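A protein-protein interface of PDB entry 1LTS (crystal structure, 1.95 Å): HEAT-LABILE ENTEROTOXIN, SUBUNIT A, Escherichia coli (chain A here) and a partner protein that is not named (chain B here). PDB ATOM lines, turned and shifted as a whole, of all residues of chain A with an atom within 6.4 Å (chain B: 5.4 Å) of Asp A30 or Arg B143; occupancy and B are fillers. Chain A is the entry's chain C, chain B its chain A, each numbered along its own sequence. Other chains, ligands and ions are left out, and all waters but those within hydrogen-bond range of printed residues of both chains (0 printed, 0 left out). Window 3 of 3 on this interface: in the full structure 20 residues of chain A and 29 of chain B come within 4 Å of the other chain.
NE of Arg B143 is in hydrogen-bond range of OE1 of Gln A26 (3.4 Å). The guanidinium group (NH2) of Arg B143 is in salt-bridge range of the side-chain carboxylate (OD1) of Asp A30 (3.0 Å).
O of Ser B119 sits at hydrogen-bond distance from N of Arg B143 (3.2 Å).
Gln A26 touches Tyr B146 (NE2 to CD1, 3.4 Å). Ile A27 touches Ser B119 (CG2 to OG, 3.9 Å). Ile A27 touches Arg B143 (CA to NH1, 3.9 Å).
Asp A30 touches one residue of chain B. Of the printed residues of chain A, Arg B143 touches Gln A26 (3.4 Å), Ile A27 (3.9 Å) and Asp A30 (3.0 Å). Of the printed residues of chain A, Tyr B146 touches Gln A26 (3.4 Å). Of the printed residues of chain B, Gln A26 touches Arg B143 (3.4 Å) and Tyr B146 (3.4 Å). Tyr B142 touches none of the printed residues of chain A. The nearest residue of chain A that does not touch Arg B143 is Val A23 (5.8 Å). The nearest printed residue of chain B that does not touch Gln A26 is Ser B119 (5.8 Å).
Hydrophobic or aromatic side chains of chain B that line the printed part of chain A: Tyr B146. Of the 10 printed residues of chain A, 3 touch a printed residue of chain B.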
ATOM      1  N   VAL A  23       5.356 -12.607   7.183  1.00  0.00           N
ATOM      2  CA  VAL A  23       4.315 -12.309   8.136  1.00  0.00           C
ATOM      3  C   VAL A  23       3.015 -12.868   7.563  1.00  0.00           C
ATOM      4  O   VAL A  23       2.270 -13.470   8.341  1.00  0.00           O
ATOM      5  CB  VAL A  23       4.239 -10.757   8.389  1.00  0.00           C
ATOM      6  CG1 VAL A  23       3.030 -10.353   9.241  1.00  0.00           C
ATOM      7  CG2 VAL A  23       5.471 -10.356   9.167  1.00  0.00           C
ATOM      8  N   ARG A  25       2.713 -15.489   5.521  1.00  0.00           N
ATOM      9  CA  ARG A  25       2.848 -16.924   5.708  1.00  0.00           C
ATOM     10  C   ARG A  25       2.520 -17.406   7.132  1.00  0.00           C
ATOM     11  O   ARG A  25       2.044 -18.522   7.351  1.00  0.00           O
ATOM     12  CB  ARG A  25       4.262 -17.319   5.329  1.00  0.00           C
ATOM     13  CG  ARG A  25       4.447 -17.386   3.806  1.00  0.00           C
ATOM     14  CD  ARG A  25       5.943 -17.427   3.472  1.00  0.00           C
ATOM     15  NE  ARG A  25       6.528 -18.693   3.814  1.00  0.00           N
ATOM     16  CZ  ARG A  25       7.758 -19.040   3.486  1.00  0.00           C
ATOM     17  NH1 ARG A  25       8.588 -18.248   2.785  1.00  0.00           N
ATOM     18  NH2 ARG A  25       8.191 -20.215   3.909  1.00  0.00           N
ATOM     19  N   GLN A  26       2.760 -16.592   8.153  1.00  0.00           N
ATOM     20  CA  GLN A  26       2.376 -16.898   9.508  1.00  0.00           C
ATOM     21  C   GLN A  26       0.892 -16.691   9.730  1.00  0.00           C
ATOM     22  O   GLN A  26       0.159 -17.626  10.051  1.00  0.00           O
ATOM     23  CB  GLN A  26       3.148 -16.005  10.459  1.00  0.00           C
ATOM     24  CG  GLN A  26       4.597 -16.383  10.544  1.00  0.00           C
ATOM     25  CD  GLN A  26       4.769 -17.807  11.002  1.00  0.00           C
ATOM     26  OE1 GLN A  26       4.203 -18.218  12.012  1.00  0.00           O
ATOM     27  NE2 GLN A  26       5.531 -18.615  10.295  1.00  0.00           N
ATOM     28  N   ILE A  27       0.365 -15.492   9.538  1.00  0.00           N
ATOM     29  CA  ILE A  27      -1.031 -15.245   9.863  1.00  0.00           C
ATOM     30  C   ILE A  27      -2.072 -15.855   8.891  1.00  0.00           C
ATOM     31  O   ILE A  27      -3.143 -16.276   9.360  1.00  0.00           O
ATOM     32  CB  ILE A  27      -1.253 -13.693  10.022  1.00  0.00           C
ATOM     33  CG1 ILE A  27      -0.886 -12.894   8.779  1.00  0.00           C
ATOM     34  CG2 ILE A  27      -0.384 -13.230  11.220  1.00  0.00           C
ATOM     35  CD1 ILE A  27      -1.098 -11.364   8.891  1.00  0.00           C
ATOM     36  N   PHE A  28      -1.829 -16.033   7.565  1.00  0.00           N
ATOM     37  CA  PHE A  28      -2.814 -16.555   6.607  1.00  0.00           C
ATOM     38  C   PHE A  28      -2.892 -18.055   6.608  1.00  0.00           C
ATOM     39  O   PHE A  28      -3.936 -18.635   6.332  1.00  0.00           O
ATOM     40  CB  PHE A  28      -2.477 -16.055   5.191  1.00  0.00           C
ATOM     41  CG  PHE A  28      -2.798 -14.569   4.987  1.00  0.00           C
ATOM     42  CD1 PHE A  28      -3.324 -13.776   6.005  1.00  0.00           C
ATOM     43  CD2 PHE A  28      -2.615 -14.007   3.748  1.00  0.00           C
ATOM     44  CE1 PHE A  28      -3.665 -12.455   5.789  1.00  0.00           C
ATOM     45  CE2 PHE A  28      -2.960 -12.683   3.529  1.00  0.00           C
ATOM     46  CZ  PHE A  28      -3.485 -11.897   4.539  1.00  0.00           C
ATOM     47  N   SER A  29      -1.802 -18.697   6.975  1.00  0.00           N
ATOM     48  CA  SER A  29      -1.771 -20.132   7.077  1.00  0.00           C
ATOM     49  C   SER A  29      -2.704 -20.627   8.159  1.00  0.00           C
ATOM     50  O   SER A  29      -3.067 -21.798   8.115  1.00  0.00           O
ATOM     51  CB  SER A  29      -0.357 -20.611   7.378  1.00  0.00           C
ATOM     52  OG  SER A  29       0.429 -20.455   6.181  1.00  0.00           O
ATOM     53  N   ASP A  30      -3.133 -19.797   9.131  1.00  0.00           N
ATOM     54  CA  ASP A  30      -4.122 -20.234  10.124  1.00  0.00           C
ATOM     55  C   ASP A  30      -5.481 -20.514   9.498  1.00  0.00           C
ATOM     56  O   ASP A  30      -6.325 -21.157  10.117  1.00  0.00           O
ATOM     57  CB  ASP A  30      -4.390 -19.188  11.229  1.00  0.00           C
ATOM     58  CG  ASP A  30      -3.235 -18.922  12.196  1.00  0.00           C
ATOM     59  OD1 ASP A  30      -2.251 -19.664  12.196  1.00  0.00           O
ATOM     60  OD2 ASP A  30      -3.332 -17.961  12.955  1.00  0.00           O
ATOM     61  N   TYR A  31      -5.702 -19.933   8.320  1.00  0.00           N
ATOM     62  CA  TYR A  31      -6.938 -20.059   7.598  1.00  0.00           C
ATOM     63  C   TYR A  31      -6.966 -21.194   6.567  1.00  0.00           C
ATOM     64  O   TYR A  31      -8.027 -21.521   6.027  1.00  0.00           O
ATOM     65  CB  TYR A  31      -7.223 -18.716   6.927  1.00  0.00           C
ATOM     66  CG  TYR A  31      -7.339 -17.583   7.927  1.00  0.00           C
ATOM     67  CD1 TYR A  31      -8.387 -17.550   8.829  1.00  0.00           C
ATOM     68  CD2 TYR A  31      -6.414 -16.570   7.902  1.00  0.00           C
ATOM     69  CE1 TYR A  31      -8.541 -16.504   9.712  1.00  0.00           C
ATOM     70  CE2 TYR A  31      -6.549 -15.522   8.783  1.00  0.00           C
ATOM     71  CZ  TYR A  31      -7.606 -15.480   9.682  1.00  0.00           C
ATOM     72  OH  TYR A  31      -7.713 -14.401  10.567  1.00  0.00           O
ATOM     73  N   GLN A  32      -5.832 -21.843   6.335  1.00  0.00           N
ATOM     74  CA  GLN A  32      -5.707 -22.852   5.312  1.00  0.00           C
ATOM     75  C   GLN A  32      -6.334 -24.121   5.827  1.00  0.00           C
ATOM     76  O   GLN A  32      -5.886 -24.608   6.871  1.00  0.00           O
ATOM     77  CB  GLN A  32      -4.233 -23.064   5.004  1.00  0.00           C
ATOM     78  CG  GLN A  32      -3.766 -24.307   4.246  1.00  0.00           C
ATOM     79  CD  GLN A  32      -4.343 -24.523   2.867  1.00  0.00           C
ATOM     80  OE1 GLN A  32      -4.369 -25.649   2.390  1.00  0.00           O
ATOM     81  NE2 GLN A  32      -4.849 -23.548   2.161  1.00  0.00           N
ATOM     82  N   SER A  33      -7.304 -24.647   5.061  1.00  0.00           N
ATOM     83  CA  SER A  33      -8.031 -25.839   5.459  1.00  0.00           C
ATOM     84  C   SER A  33      -7.806 -26.939   4.410  1.00  0.00           C
ATOM     85  O   SER A  33      -8.109 -26.780   3.233  1.00  0.00           O
ATOM     86  CB  SER A  33      -9.515 -25.453   5.604  1.00  0.00           C
ATOM     87  OG  SER A  33     -10.367 -26.435   6.213  1.00  0.00           O
ATOM     88  N   SER B 119       1.392  -9.144  15.187  1.00  0.00           N
ATOM     89  CA  SER B 119       1.838 -10.438  15.706  1.00  0.00           C
ATOM     90  C   SER B 119       3.229 -10.465  16.306  1.00  0.00           C
ATOM     91  O   SER B 119       3.650 -11.434  16.935  1.00  0.00           O
ATOM     92  CB  SER B 119       1.775 -11.496  14.598  1.00  0.00           C
ATOM     93  OG  SER B 119       2.090 -11.040  13.297  1.00  0.00           O
ATOM     94  N   GLU B 141      -2.447 -12.432  19.979  1.00  0.00           N
ATOM     95  CA  GLU B 141      -2.090 -12.684  18.586  1.00  0.00           C
ATOM     96  C   GLU B 141      -0.605 -12.757  18.316  1.00  0.00           C
ATOM     97  O   GLU B 141      -0.181 -12.849  17.157  1.00  0.00           O
ATOM     98  CB  GLU B 141      -2.687 -11.628  17.715  1.00  0.00           C
ATOM     99  CG  GLU B 141      -4.149 -11.988  17.744  1.00  0.00           C
ATOM    100  CD  GLU B 141      -4.998 -10.942  17.112  1.00  0.00           C
ATOM    101  OE1 GLU B 141      -4.883 -10.765  15.898  1.00  0.00           O
ATOM    102  OE2 GLU B 141      -5.748 -10.304  17.859  1.00  0.00           O
ATOM    103  N   TYR B 142       0.180 -12.738  19.402  1.00  0.00           N
ATOM    104  CA  TYR B 142       1.622 -12.816  19.295  1.00  0.00           C
ATOM    105  C   TYR B 142       2.003 -14.225  18.807  1.00  0.00           C
ATOM    106  O   TYR B 142       1.500 -15.208  19.357  1.00  0.00           O
ATOM    107  CB  TYR B 142       2.209 -12.524  20.671  1.00  0.00           C
ATOM    108  CG  TYR B 142       3.699 -12.802  20.751  1.00  0.00           C
ATOM    109  CD1 TYR B 142       4.579 -11.961  20.086  1.00  0.00           C
ATOM    110  CD2 TYR B 142       4.146 -13.881  21.471  1.00  0.00           C
ATOM    111  CE1 TYR B 142       5.929 -12.210  20.153  1.00  0.00           C
ATOM    112  CE2 TYR B 142       5.498 -14.134  21.534  1.00  0.00           C
ATOM    113  CZ  TYR B 142       6.377 -13.297  20.877  1.00  0.00           C
ATOM    114  OH  TYR B 142       7.742 -13.554  20.946  1.00  0.00           O
ATOM    115  N   ARG B 143       2.928 -14.440  17.858  1.00  0.00           N
ATOM    116  CA  ARG B 143       3.243 -15.760  17.349  1.00  0.00           C
ATOM    117  C   ARG B 143       4.485 -16.202  18.012  1.00  0.00           C
ATOM    118  O   ARG B 143       5.595 -16.007  17.537  1.00  0.00           O
ATOM    119  CB  ARG B 143       3.429 -15.703  15.854  1.00  0.00           C
ATOM    120  CG  ARG B 143       2.139 -15.114  15.299  1.00  0.00           C
ATOM    121  CD  ARG B 143       1.922 -15.376  13.843  1.00  0.00           C
ATOM    122  NE  ARG B 143       1.649 -16.798  13.685  1.00  0.00           N
ATOM    123  CZ  ARG B 143       0.407 -17.285  13.552  1.00  0.00           C
ATOM    124  NH1 ARG B 143      -0.684 -16.500  13.546  1.00  0.00           N
ATOM    125  NH2 ARG B 143       0.282 -18.609  13.460  1.00  0.00           N
ATOM    126  N   ASP B 144       4.257 -16.863  19.121  1.00  0.00           N
ATOM    127  CA  ASP B 144       5.326 -17.265  20.018  1.00  0.00           C
ATOM    128  C   ASP B 144       6.424 -18.108  19.433  1.00  0.00           C
ATOM    129  O   ASP B 144       7.604 -17.823  19.549  1.00  0.00           O
ATOM    130  CB  ASP B 144       4.737 -18.005  21.192  1.00  0.00           C
ATOM    131  CG  ASP B 144       5.627 -17.887  22.413  1.00  0.00           C
ATOM    132  OD1 ASP B 144       6.581 -18.657  22.575  1.00  0.00           O
ATOM    133  OD2 ASP B 144       5.341 -16.990  23.201  1.00  0.00           O
ATOM    134  N   ARG B 145       6.059 -19.214  18.831  1.00  0.00           N
ATOM    135  CA  ARG B 145       7.024 -20.102  18.225  1.00  0.00           C
ATOM    136  C   ARG B 145       7.774 -19.380  17.131  1.00  0.00           C
ATOM    137  O   ARG B 145       8.978 -19.564  17.042  1.00  0.00           O
ATOM    138  CB  ARG B 145       6.340 -21.338  17.617  1.00  0.00           C
ATOM    139  CG  ARG B 145       7.338 -22.387  17.114  1.00  0.00           C
ATOM    140  CD  ARG B 145       6.724 -23.510  16.275  1.00  0.00           C
ATOM    141  NE  ARG B 145       5.891 -24.354  17.085  1.00  0.00           N
ATOM    142  CZ  ARG B 145       4.565 -24.477  16.916  1.00  0.00           C
ATOM    143  NH1 ARG B 145       3.865 -23.841  15.980  1.00  0.00           N
ATOM    144  NH2 ARG B 145       3.895 -25.204  17.770  1.00  0.00           N
ATOM    145  N   TYR B 146       7.132 -18.553  16.319  1.00  0.00           N
ATOM    146  CA  TYR B 146       7.857 -17.978  15.209  1.00  0.00           C
ATOM    147  C   TYR B 146       8.924 -17.044  15.722  1.00  0.00           C
ATOM    148  O   TYR B 146      10.088 -17.188  15.374  1.00  0.00           O
ATOM    149  CB  TYR B 146       6.889 -17.238  14.293  1.00  0.00           C
ATOM    150  CG  TYR B 146       7.522 -16.723  13.006  1.00  0.00           C
ATOM    151  CD1 TYR B 146       8.218 -17.577  12.186  1.00  0.00           C
ATOM    152  CD2 TYR B 146       7.436 -15.384  12.664  1.00  0.00           C
ATOM    153  CE1 TYR B 146       8.827 -17.099  11.043  1.00  0.00           C
ATOM    154  CE2 TYR B 146       8.041 -14.894  11.520  1.00  0.00           C
ATOM    155  CZ  TYR B 146       8.738 -15.769  10.717  1.00  0.00           C
ATOM    156  OH  TYR B 146       9.372 -15.307   9.582  1.00  0.00           O
ATOM    157  N   TYR B 147       8.557 -16.124  16.591  1.00  0.00           N
ATOM    158  CA  TYR B 147       9.502 -15.137  17.070  1.00  0.00           C
ATOM    159  C   TYR B 147      10.476 -15.610  18.127  1.00  0.00           C
ATOM    160  O   TYR B 147      11.500 -14.969  18.340  1.00  0.00           O
ATOM    161  CB  TYR B 147       8.712 -13.964  17.573  1.00  0.00           C
ATOM    162  CG  TYR B 147       8.146 -13.205  16.409  1.00  0.00           C
ATOM    163  CD1 TYR B 147       9.001 -12.548  15.554  1.00  0.00           C
ATOM    164  CD2 TYR B 147       6.796 -13.235  16.203  1.00  0.00           C
ATOM    165  CE1 TYR B 147       8.484 -11.920  14.449  1.00  0.00           C
ATOM    166  CE2 TYR B 147       6.275 -12.605  15.107  1.00  0.00           C
ATOM    167  CZ  TYR B 147       7.121 -11.949  14.234  1.00  0.00           C
ATOM    168  OH  TYR B 147       6.572 -11.289  13.136  1.00  0.00           O
ATOM    169  N   ARG B 148      10.265 -16.783  18.710  1.00  0.00           N
ATOM    170  CA  ARG B 148      11.073 -17.341  19.788  1.00  0.00           C
ATOM    171  C   ARG B 148      12.567 -17.446  19.507  1.00  0.00           C
ATOM    172  O   ARG B 148      13.433 -17.213  20.348  1.00  0.00           O
ATOM    173  CB  ARG B 148      10.517 -18.733  20.138  1.00  0.00           C
ATOM    174  CG  ARG B 148      11.098 -19.493  21.358  1.00  0.00           C
ATOM    175  CD  ARG B 148      10.388 -20.831  21.596  1.00  0.00           C
ATOM    176  NE  ARG B 148       8.941 -20.659  21.663  1.00  0.00           N
ATOM    177  CZ  ARG B 148       8.090 -21.592  21.230  1.00  0.00           C
ATOM    178  NH1 ARG B 148       8.527 -22.745  20.720  1.00  0.00           N
ATOM    179  NH2 ARG B 148       6.782 -21.351  21.255  1.00  0.00           N
